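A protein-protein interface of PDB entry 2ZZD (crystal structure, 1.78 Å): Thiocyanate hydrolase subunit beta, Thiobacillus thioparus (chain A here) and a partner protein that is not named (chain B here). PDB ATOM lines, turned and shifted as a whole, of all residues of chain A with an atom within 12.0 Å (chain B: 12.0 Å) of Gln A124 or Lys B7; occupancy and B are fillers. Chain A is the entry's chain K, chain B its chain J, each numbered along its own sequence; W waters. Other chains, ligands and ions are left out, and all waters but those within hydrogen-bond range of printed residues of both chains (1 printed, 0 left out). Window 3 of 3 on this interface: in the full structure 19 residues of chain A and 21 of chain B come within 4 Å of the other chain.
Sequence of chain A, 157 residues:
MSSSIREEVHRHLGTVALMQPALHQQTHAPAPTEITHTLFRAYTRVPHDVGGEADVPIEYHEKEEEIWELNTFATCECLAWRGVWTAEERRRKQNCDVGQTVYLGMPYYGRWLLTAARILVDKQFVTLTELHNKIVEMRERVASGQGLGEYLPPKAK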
ATOM      1  N   LEU A  79      10.868 -21.179  12.932  1.00  0.00           N
ATOM      2  CA  LEU A  79      10.391 -21.836  14.141  1.00  0.00           C
ATOM      3  C   LEU A  79       9.071 -22.556  13.855  1.00  0.00           C
ATOM      4  O   LEU A  79       8.808 -23.627  14.398  1.00  0.00           O
ATOM      5  CB  LEU A  79      10.207 -20.813  15.269  1.00  0.00           C
ATOM      6  CG  LEU A  79      11.496 -20.323  15.942  1.00  0.00           C
ATOM      7  CD1 LEU A  79      11.194 -19.160  16.881  1.00  0.00           C
ATOM      8  CD2 LEU A  79      12.141 -21.471  16.716  1.00  0.00           C
ATOM      9  N   GLY A  83       8.110 -26.784  13.409  1.00  0.00           N
ATOM     10  CA  GLY A  83       7.225 -27.271  14.459  1.00  0.00           C
ATOM     11  C   GLY A  83       7.244 -26.755  15.889  1.00  0.00           C
ATOM     12  O   GLY A  83       6.597 -27.352  16.755  1.00  0.00           O
ATOM     13  N   VAL A  84       7.965 -25.673  16.161  1.00  0.00           N
ATOM     14  CA  VAL A  84       8.000 -25.123  17.516  1.00  0.00           C
ATOM     15  C   VAL A  84       6.641 -24.482  17.837  1.00  0.00           C
ATOM     16  O   VAL A  84       6.191 -24.480  18.991  1.00  0.00           O
ATOM     17  CB  VAL A  84       9.145 -24.097  17.649  1.00  0.00           C
ATOM     18  CG1 VAL A  84       8.976 -23.261  18.913  1.00  0.00           C
ATOM     19  CG2 VAL A  84      10.482 -24.840  17.694  1.00  0.00           C
ATOM     20  N   TRP A  85       5.998 -23.947  16.801  1.00  0.00           N
ATOM     21  CA  TRP A  85       4.673 -23.338  16.915  1.00  0.00           C
ATOM     22  C   TRP A  85       4.006 -23.210  15.548  1.00  0.00           C
ATOM     23  O   TRP A  85       4.645 -23.424  14.519  1.00  0.00           O
ATOM     24  CB  TRP A  85       4.746 -21.946  17.587  1.00  0.00           C
ATOM     25  CG  TRP A  85       5.579 -20.864  16.899  1.00  0.00           C
ATOM     26  CD1 TRP A  85       6.233 -20.944  15.696  1.00  0.00           C
ATOM     27  CD2 TRP A  85       5.877 -19.559  17.425  1.00  0.00           C
ATOM     28  NE1 TRP A  85       6.921 -19.773  15.449  1.00  0.00           N
ATOM     29  CE2 TRP A  85       6.719 -18.911  16.494  1.00  0.00           C
ATOM     30  CE3 TRP A  85       5.510 -18.877  18.595  1.00  0.00           C
ATOM     31  CZ2 TRP A  85       7.211 -17.612  16.703  1.00  0.00           C
ATOM     32  CZ3 TRP A  85       5.998 -17.580  18.801  1.00  0.00           C
ATOM     33  CH2 TRP A  85       6.840 -16.966  17.857  1.00  0.00           C
ATOM     34  N   GLU A  89      -0.437 -19.723  16.947  1.00  0.00           N
ATOM     35  CA  GLU A  89       0.082 -19.643  18.304  1.00  0.00           C
ATOM     36  C   GLU A  89       0.941 -18.376  18.377  1.00  0.00           C
ATOM     37  O   GLU A  89       0.902 -17.650  19.369  1.00  0.00           O
ATOM     38  CB  GLU A  89       0.906 -20.893  18.644  1.00  0.00           C
ATOM     39  CG  GLU A  89       0.059 -22.165  18.750  1.00  0.00           C
ATOM     40  CD  GLU A  89       0.880 -23.416  19.014  1.00  0.00           C
ATOM     41  OE1 GLU A  89       1.832 -23.675  18.250  1.00  0.00           O
ATOM     42  OE2 GLU A  89       0.567 -24.148  19.978  1.00  0.00           O
ATOM     43  N   ARG A  92      -1.357 -15.158  18.603  1.00  0.00           N
ATOM     44  CA  ARG A  92      -1.966 -15.027  19.915  1.00  0.00           C
ATOM     45  C   ARG A  92      -0.948 -14.500  20.930  1.00  0.00           C
ATOM     46  O   ARG A  92      -1.258 -13.615  21.724  1.00  0.00           O
ATOM     47  CB  ARG A  92      -2.533 -16.381  20.358  1.00  0.00           C
ATOM     48  CG  ARG A  92      -3.189 -16.388  21.733  1.00  0.00           C
ATOM     49  CD  ARG A  92      -2.203 -16.816  22.805  1.00  0.00           C
ATOM     50  NE  ARG A  92      -1.744 -18.184  22.595  1.00  0.00           N
ATOM     51  CZ  ARG A  92      -0.885 -18.810  23.394  1.00  0.00           C
ATOM     52  NH1 ARG A  92      -0.389 -18.183  24.455  1.00  0.00           N
ATOM     53  NH2 ARG A  92      -0.528 -20.066  23.143  1.00  0.00           N
ATOM     54  N   LYS A  93       0.273 -15.027  20.891  1.00  0.00           N
ATOM     55  CA  LYS A  93       1.311 -14.599  21.828  1.00  0.00           C
ATOM     56  C   LYS A  93       1.872 -13.206  21.521  1.00  0.00           C
ATOM     57  O   LYS A  93       2.117 -12.400  22.423  1.00  0.00           O
ATOM     58  CB  LYS A  93       2.478 -15.602  21.817  1.00  0.00           C
ATOM     59  CG  LYS A  93       2.125 -17.000  22.318  1.00  0.00           C
ATOM     60  CD  LYS A  93       3.328 -17.953  22.223  1.00  0.00           C
ATOM     61  CE  LYS A  93       4.384 -17.648  23.280  1.00  0.00           C
ATOM     62  NZ  LYS A  93       3.862 -17.887  24.662  1.00  0.00           N
ATOM     63  N   THR A 115       8.464 -12.091  21.095  1.00  0.00           N
ATOM     64  CA  THR A 115       7.645 -13.290  21.117  1.00  0.00           C
ATOM     65  C   THR A 115       8.408 -14.527  20.665  1.00  0.00           C
ATOM     66  O   THR A 115       8.109 -15.630  21.110  1.00  0.00           O
ATOM     67  CB  THR A 115       6.372 -13.075  20.286  1.00  0.00           C
ATOM     68  OG1 THR A 115       5.703 -11.898  20.766  1.00  0.00           O
ATOM     69  CG2 THR A 115       5.433 -14.266  20.420  1.00  0.00           C
ATOM     70  N   ALA A 116       9.397 -14.351  19.793  1.00  0.00           N
ATOM     71  CA  ALA A 116      10.199 -15.486  19.351  1.00  0.00           C
ATOM     72  C   ALA A 116      10.997 -15.954  20.571  1.00  0.00           C
ATOM     73  O   ALA A 116      11.155 -17.151  20.810  1.00  0.00           O
ATOM     74  CB  ALA A 116      11.145 -15.069  18.222  1.00  0.00           C
ATOM     75  N   ALA A 117      11.496 -14.995  21.346  1.00  0.00           N
ATOM     76  CA  ALA A 117      12.258 -15.318  22.545  1.00  0.00           C
ATOM     77  C   ALA A 117      11.327 -16.000  23.541  1.00  0.00           C
ATOM     78  O   ALA A 117      11.701 -16.960  24.216  1.00  0.00           O
ATOM     79  CB  ALA A 117      12.834 -14.043  23.164  1.00  0.00           C
ATOM     80  N   ARG A 118      10.101 -15.494  23.611  1.00  0.00           N
ATOM     81  CA  ARG A 118       9.092 -16.004  24.522  1.00  0.00           C
ATOM     82  C   ARG A 118       8.728 -17.474  24.289  1.00  0.00           C
ATOM     83  O   ARG A 118       8.649 -18.256  25.243  1.00  0.00           O
ATOM     84  CB  ARG A 118       7.843 -15.130  24.415  1.00  0.00           C
ATOM     85  CG  ARG A 118       6.827 -15.365  25.499  1.00  0.00           C
ATOM     86  CD  ARG A 118       7.239 -14.767  26.837  1.00  0.00           C
ATOM     87  NE  ARG A 118       6.576 -15.505  27.903  1.00  0.00           N
ATOM     88  CZ  ARG A 118       6.240 -15.011  29.089  1.00  0.00           C
ATOM     89  NH1 ARG A 118       6.499 -13.746  29.397  1.00  0.00           N
ATOM     90  NH2 ARG A 118       5.638 -15.797  29.971  1.00  0.00           N
ATOM     91  N   ILE A 119       8.506 -17.868  23.037  1.00  0.00           N
ATOM     92  CA  ILE A 119       8.135 -19.255  22.783  1.00  0.00           C
ATOM     93  C   ILE A 119       9.252 -20.219  23.195  1.00  0.00           C
ATOM     94  O   ILE A 119       8.978 -21.330  23.640  1.00  0.00           O
ATOM     95  CB  ILE A 119       7.736 -19.480  21.292  1.00  0.00           C
ATOM     96  CG1 ILE A 119       7.090 -20.859  21.123  1.00  0.00           C
ATOM     97  CG2 ILE A 119       8.951 -19.343  20.385  1.00  0.00           C
ATOM     98  CD1 ILE A 119       5.742 -20.992  21.814  1.00  0.00           C
ATOM     99  N   LEU A 120      10.506 -19.795  23.066  1.00  0.00           N
ATOM    100  CA  LEU A 120      11.619 -20.657  23.460  1.00  0.00           C
ATOM    101  C   LEU A 120      11.558 -20.960  24.957  1.00  0.00           C
ATOM    102  O   LEU A 120      11.851 -22.075  25.388  1.00  0.00           O
ATOM    103  CB  LEU A 120      12.965 -19.993  23.146  1.00  0.00           C
ATOM    104  CG  LEU A 120      13.290 -19.672  21.685  1.00  0.00           C
ATOM    105  CD1 LEU A 120      14.731 -19.185  21.590  1.00  0.00           C
ATOM    106  CD2 LEU A 120      13.096 -20.906  20.822  1.00  0.00           C
ATOM    107  N   VAL A 121      11.176 -19.957  25.744  1.00  0.00           N
ATOM    108  CA  VAL A 121      11.088 -20.112  27.190  1.00  0.00           C
ATOM    109  C   VAL A 121       9.790 -20.777  27.653  1.00  0.00           C
ATOM    110  O   VAL A 121       9.815 -21.657  28.517  1.00  0.00           O
ATOM    111  CB  VAL A 121      11.234 -18.748  27.903  1.00  0.00           C
ATOM    112  CG1 VAL A 121      11.070 -18.922  29.403  1.00  0.00           C
ATOM    113  CG2 VAL A 121      12.604 -18.149  27.596  1.00  0.00           C
ATOM    114  N   ASP A 122       8.660 -20.365  27.091  1.00  0.00           N
ATOM    115  CA  ASP A 122       7.388 -20.951  27.496  1.00  0.00           C
ATOM    116  C   ASP A 122       7.280 -22.443  27.184  1.00  0.00           C
ATOM    117  O   ASP A 122       6.647 -23.184  27.932  1.00  0.00           O
ATOM    118  CB  ASP A 122       6.212 -20.203  26.864  1.00  0.00           C
ATOM    119  CG  ASP A 122       5.953 -18.860  27.526  1.00  0.00           C
ATOM    120  OD1 ASP A 122       6.151 -18.761  28.757  1.00  0.00           O
ATOM    121  OD2 ASP A 122       5.538 -17.910  26.826  1.00  0.00           O
ATOM    122  N   LYS A 123       7.890 -22.895  26.090  1.00  0.00           N
ATOM    123  CA  LYS A 123       7.824 -24.318  25.761  1.00  0.00           C
ATOM    124  C   LYS A 123       9.054 -25.073  26.277  1.00  0.00           C
ATOM    125  O   LYS A 123       9.301 -26.225  25.911  1.00  0.00           O
ATOM    126  CB  LYS A 123       7.616 -24.519  24.253  1.00  0.00           C
ATOM    127  CG  LYS A 123       6.133 -24.370  23.856  1.00  0.00           C
ATOM    128  CD  LYS A 123       5.838 -24.625  22.379  1.00  0.00           C
ATOM    129  CE  LYS A 123       4.329 -24.509  22.128  1.00  0.00           C
ATOM    130  NZ  LYS A 123       3.965 -24.376  20.683  1.00  0.00           N
ATOM    131  N   GLN A 124       9.806 -24.403  27.146  1.00  0.00           N
ATOM    132  CA  GLN A 124      10.990 -24.968  27.793  1.00  0.00           C
ATOM    133  C   GLN A 124      12.108 -25.507  26.897  1.00  0.00           C
ATOM    134  O   GLN A 124      12.817 -26.450  27.268  1.00  0.00           O
ATOM    135  CB  GLN A 124      10.542 -26.029  28.812  1.00  0.00           C
ATOM    136  CG  GLN A 124       9.834 -25.394  30.024  1.00  0.00           C
ATOM    137  CD  GLN A 124       9.144 -26.391  30.945  1.00  0.00           C
ATOM    138  OE1 GLN A 124       8.114 -26.967  30.599  1.00  0.00           O
ATOM    139  NE2 GLN A 124       9.711 -26.591  32.128  1.00  0.00           N
ATOM    140  N   PHE A 125      12.276 -24.897  25.726  1.00  0.00           N
ATOM    141  CA  PHE A 125      13.350 -25.295  24.821  1.00  0.00           C
ATOM    142  C   PHE A 125      14.649 -24.670  25.357  1.00  0.00           C
ATOM    143  O   PHE A 125      15.743 -25.191  25.131  1.00  0.00           O
ATOM    144  CB  PHE A 125      13.033 -24.858  23.385  1.00  0.00           C
ATOM    145  CG  PHE A 125      11.933 -25.673  22.740  1.00  0.00           C
ATOM    146  CD1 PHE A 125      12.067 -27.052  22.600  1.00  0.00           C
ATOM    147  CD2 PHE A 125      10.753 -25.073  22.304  1.00  0.00           C
ATOM    148  CE1 PHE A 125      11.041 -27.824  22.038  1.00  0.00           C
ATOM    149  CE2 PHE A 125       9.722 -25.837  21.741  1.00  0.00           C
ATOM    150  CZ  PHE A 125       9.871 -27.214  21.612  1.00  0.00           C
ATOM    151  N   VAL A 126      14.512 -23.551  26.068  1.00  0.00           N
ATOM    152  CA  VAL A 126      15.641 -22.891  26.731  1.00  0.00           C
ATOM    153  C   VAL A 126      15.079 -22.415  28.066  1.00  0.00           C
ATOM    154  O   VAL A 126      13.874 -22.173  28.178  1.00  0.00           O
ATOM    155  CB  VAL A 126      16.188 -21.626  25.983  1.00  0.00           C
ATOM    156  CG1 VAL A 126      16.494 -21.946  24.531  1.00  0.00           C
ATOM    157  CG2 VAL A 126      15.210 -20.463  26.112  1.00  0.00           C
ATOM    158  N   THR A 127      15.929 -22.310  29.082  1.00  0.00           N
ATOM    159  CA  THR A 127      15.470 -21.819  30.379  1.00  0.00           C
ATOM    160  C   THR A 127      15.601 -20.306  30.300  1.00  0.00           C
ATOM    161  O   THR A 127      16.290 -19.789  29.424  1.00  0.00           O
ATOM    162  CB  THR A 127      16.359 -22.314  31.537  1.00  0.00           C
ATOM    163  OG1 THR A 127      17.692 -21.813  31.367  1.00  0.00           O
ATOM    164  CG2 THR A 127      16.376 -23.833  31.581  1.00  0.00           C
ATOM    165  N   LEU A 128      14.937 -19.587  31.199  1.00  0.00           N
ATOM    166  CA  LEU A 128      15.051 -18.140  31.168  1.00  0.00           C
ATOM    167  C   LEU A 128      16.498 -17.784  31.485  1.00  0.00           C
ATOM    168  O   LEU A 128      17.026 -16.790  30.992  1.00  0.00           O
ATOM    169  CB  LEU A 128      14.115 -17.489  32.189  1.00  0.00           C
ATOM    170  CG  LEU A 128      14.115 -15.957  32.167  1.00  0.00           C
ATOM    171  CD1 LEU A 128      13.690 -15.459  30.788  1.00  0.00           C
ATOM    172  CD2 LEU A 128      13.170 -15.428  33.237  1.00  0.00           C
ATOM    173  N   THR A 129      17.132 -18.610  32.314  1.00  0.00           N
ATOM    174  CA  THR A 129      18.521 -18.389  32.695  1.00  0.00           C
ATOM    175  C   THR A 129      19.416 -18.456  31.455  1.00  0.00           C
ATOM    176  O   THR A 129      20.313 -17.629  31.279  1.00  0.00           O
ATOM    177  CB  THR A 129      18.982 -19.427  33.743  1.00  0.00           C
ATOM    178  OG1 THR A 129      18.154 -19.323  34.910  1.00  0.00           O
ATOM    179  CG2 THR A 129      20.433 -19.180  34.145  1.00  0.00           C
ATOM    180  N   GLU A 130      19.164 -19.429  30.584  1.00  0.00           N
ATOM    181  CA  GLU A 130      19.950 -19.548  29.362  1.00  0.00           C
ATOM    182  C   GLU A 130      19.749 -18.313  28.485  1.00  0.00           C
ATOM    183  O   GLU A 130      20.691 -17.831  27.854  1.00  0.00           O
ATOM    184  CB  GLU A 130      19.562 -20.814  28.589  1.00  0.00           C
ATOM    185  CG  GLU A 130      20.101 -22.097  29.211  1.00  0.00           C
ATOM    186  CD  GLU A 130      19.643 -23.343  28.470  1.00  0.00           C
ATOM    187  OE1 GLU A 130      18.425 -23.469  28.229  1.00  0.00           O
ATOM    188  OE2 GLU A 130      20.492 -24.198  28.137  1.00  0.00           O
ATOM    189  N   LEU A 131      18.526 -17.789  28.451  1.00  0.00           N
ATOM    190  CA  LEU A 131      18.256 -16.600  27.650  1.00  0.00           C
ATOM    191  C   LEU A 131      18.975 -15.393  28.254  1.00  0.00           C
ATOM    192  O   LEU A 131      19.624 -14.632  27.539  1.00  0.00           O
ATOM    193  CB  LEU A 131      16.754 -16.317  27.568  1.00  0.00           C
ATOM    194  CG  LEU A 131      16.361 -15.057  26.780  1.00  0.00           C
ATOM    195  CD1 LEU A 131      16.886 -15.147  25.352  1.00  0.00           C
ATOM    196  CD2 LEU A 131      14.847 -14.903  26.777  1.00  0.00           C
ATOM    197  N   LYS B   7       8.962 -33.673  32.486  1.00  0.00           N
ATOM    198  CA  LYS B   7       8.843 -32.443  31.645  1.00  0.00           C
ATOM    199  C   LYS B   7       8.058 -32.795  30.383  1.00  0.00           C
ATOM    200  O   LYS B   7       8.268 -33.855  29.793  1.00  0.00           O
ATOM    201  CB  LYS B   7      10.235 -31.927  31.267  1.00  0.00           C
ATOM    202  CG  LYS B   7      10.249 -30.474  30.807  1.00  0.00           C
ATOM    203  CD  LYS B   7      11.640 -29.983  30.396  1.00  0.00           C
ATOM    204  CE  LYS B   7      12.118 -30.616  29.092  1.00  0.00           C
ATOM    205  NZ  LYS B   7      12.885 -29.644  28.254  1.00  0.00           N
ATOM    206  N   PRO B   8       7.155 -31.904  29.942  1.00  0.00           N
ATOM    207  CA  PRO B   8       6.366 -32.186  28.740  1.00  0.00           C
ATOM    208  C   PRO B   8       7.218 -32.215  27.484  1.00  0.00           C
ATOM    209  O   PRO B   8       8.218 -31.504  27.381  1.00  0.00           O
ATOM    210  CB  PRO B   8       5.360 -31.032  28.676  1.00  0.00           C
ATOM    211  CG  PRO B   8       5.593 -30.232  29.915  1.00  0.00           C
ATOM    212  CD  PRO B   8       6.987 -30.504  30.353  1.00  0.00           C
ATOM    213  N   VAL B   9       6.810 -33.043  26.531  1.00  0.00           N
ATOM    214  CA  VAL B   9       7.509 -33.145  25.263  1.00  0.00           C
ATOM    215  C   VAL B   9       6.587 -32.579  24.191  1.00  0.00           C
ATOM    216  O   VAL B   9       5.396 -32.893  24.152  1.00  0.00           O
ATOM    217  CB  VAL B   9       7.847 -34.605  24.904  1.00  0.00           C
ATOM    218  CG1 VAL B   9       8.576 -34.651  23.570  1.00  0.00           C
ATOM    219  CG2 VAL B   9       8.708 -35.227  25.991  1.00  0.00           C
ATOM    220  N   TRP B  10       7.141 -31.726  23.340  1.00  0.00           N
ATOM    221  CA  TRP B  10       6.377 -31.117  22.267  1.00  0.00           C
ATOM    222  C   TRP B  10       6.616 -31.867  20.976  1.00  0.00           C
ATOM    223  O   TRP B  10       7.758 -32.159  20.621  1.00  0.00           O
ATOM    224  CB  TRP B  10       6.779 -29.656  22.094  1.00  0.00           C
ATOM    225  CG  TRP B  10       6.552 -28.901  23.335  1.00  0.00           C
ATOM    226  CD1 TRP B  10       7.467 -28.628  24.310  1.00  0.00           C
ATOM    227  CD2 TRP B  10       5.291 -28.450  23.828  1.00  0.00           C
ATOM    228  NE1 TRP B  10       6.851 -28.045  25.386  1.00  0.00           N
ATOM    229  CE2 TRP B  10       5.513 -27.922  25.118  1.00  0.00           C
ATOM    230  CE3 TRP B  10       3.989 -28.445  23.308  1.00  0.00           C
ATOM    231  CZ2 TRP B  10       4.481 -27.395  25.898  1.00  0.00           C
ATOM    232  CZ3 TRP B  10       2.963 -27.921  24.084  1.00  0.00           C
ATOM    233  CH2 TRP B  10       3.217 -27.403  25.366  1.00  0.00           C
ATOM    234  N   ASP B  11       5.532 -32.188  20.281  1.00  0.00           N
ATOM    235  CA  ASP B  11       5.638 -32.899  19.020  1.00  0.00           C
ATOM    236  C   ASP B  11       5.924 -31.880  17.930  1.00  0.00           C
ATOM    237  O   ASP B  11       5.019 -31.185  17.470  1.00  0.00           O
ATOM    238  CB  ASP B  11       4.336 -33.618  18.705  1.00  0.00           C
ATOM    239  CG  ASP B  11       4.441 -34.476  17.467  1.00  0.00           C
ATOM    240  OD1 ASP B  11       5.334 -34.215  16.633  1.00  0.00           O
ATOM    241  OD2 ASP B  11       3.622 -35.404  17.317  1.00  0.00           O
ATOM    242  N   ARG B  12       7.172 -31.797  17.497  1.00  0.00           N
ATOM    243  CA  ARG B  12       7.509 -30.813  16.483  1.00  0.00           C
ATOM    244  C   ARG B  12       7.425 -31.314  15.036  1.00  0.00           C
ATOM    245  O   ARG B  12       7.783 -30.588  14.106  1.00  0.00           O
ATOM    246  CB  ARG B  12       8.892 -30.227  16.788  1.00  0.00           C
ATOM    247  CG  ARG B  12       9.053 -29.794  18.256  1.00  0.00           C
ATOM    248  CD  ARG B  12      10.087 -28.689  18.426  1.00  0.00           C
ATOM    249  NE  ARG B  12      11.346 -28.970  17.739  1.00  0.00           N
ATOM    250  CZ  ARG B  12      12.355 -29.671  18.247  1.00  0.00           C
ATOM    251  NH1 ARG B  12      12.274 -30.180  19.467  1.00  0.00           N
ATOM    252  NH2 ARG B  12      13.453 -29.847  17.529  1.00  0.00           N
HETATM  253  O   HOH W   1       6.748 -26.814  28.394  1.00  0.00           O
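Printed residues of chain A that touch a printed residue of chain B: Gly A83, Val A84, Lys A123, Gln A124 and Phe A125. Hydrophobic or aromatic side chains of chain A that line the printed part of chain B: Val A84 and Phe A125. Printed residues of chain B that touch a printed residue of chain A: Lys B7, Pro B8, Trp B10 and Arg B12. Hydrophobic or aromatic side chains of chain B that line the printed part of chain A: Pro B8 and Trp B10. Among the printed residues, 7 pairs touch across the chains.
O of Gln A124 is in hydrogen-bond range of NZ of Lys B7, at 3.3 Å. NE1 of Trp B10 lies within hydrogen-bond range of O of Lys A123 (3.1 Å).
Among the printed residues, merely in contact across the chains: Gly A83 with Arg B12 (3.4 Å), Val A84 with Arg B12 (3.9 Å), Gln A124 with Pro B8 (3.7 Å), Phe A125 with Trp B10 (3.9 Å) and Phe A125 with Arg B12 (3.5 Å).
The backbone carbonyl oxygen (O) of Leu A79 sits at hydrogen-bond distance from the backbone NH (N) of Val A84. The side-chain amino group (NZ) of Lys A123 sits at hydrogen-bond distance from the backbone carbonyl oxygen (O) of Val A84, 2.8 Å away. OE1 of Glu A89 lies within salt-bridge range of NZ of Lys A123 (3.3 Å). The backbone NH of Phe A125 sits at hydrogen-bond distance from the backbone carbonyl oxygen of Leu A120.
Water W1 lies within hydrogen-bond range of the side-chain amide oxygen of Gln A124 (2.6 Å) and the indole nitrogen of Trp B10 (3.3 Å).
Gln A124 touches two residues of chain B. Of chain A, only Gln A124 (3.3 Å) comes within 4 Å of Lys B7. No residue of chain B comes within 4 Å of Asp A122. Phe A125 touches two residues of chain B. No residue of chain B comes within 4 Å of Thr A127. Val B9 touches none of the printed residues of chain A. Printed residues of chain B within 4 Å of Gly A83: Arg B12. Printed residues of chain B within 4 Å of Lys A123: Trp B10 (3.1 Å). Printed residues of chain B within 4 Å of Val A84: Arg B12. Of the printed residues of chain A, Trp B10 touches Lys A123 (3.1 Å) and Phe A125 (3.9 Å). Leu A79 touches none of the printed residues of chain B. The nearest residue of chain B that does not touch Gln A124 is Trp B10 (5.0 Å). The nearest residue of chain A that does not touch Lys B7 is Phe A125 (5.4 Å).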
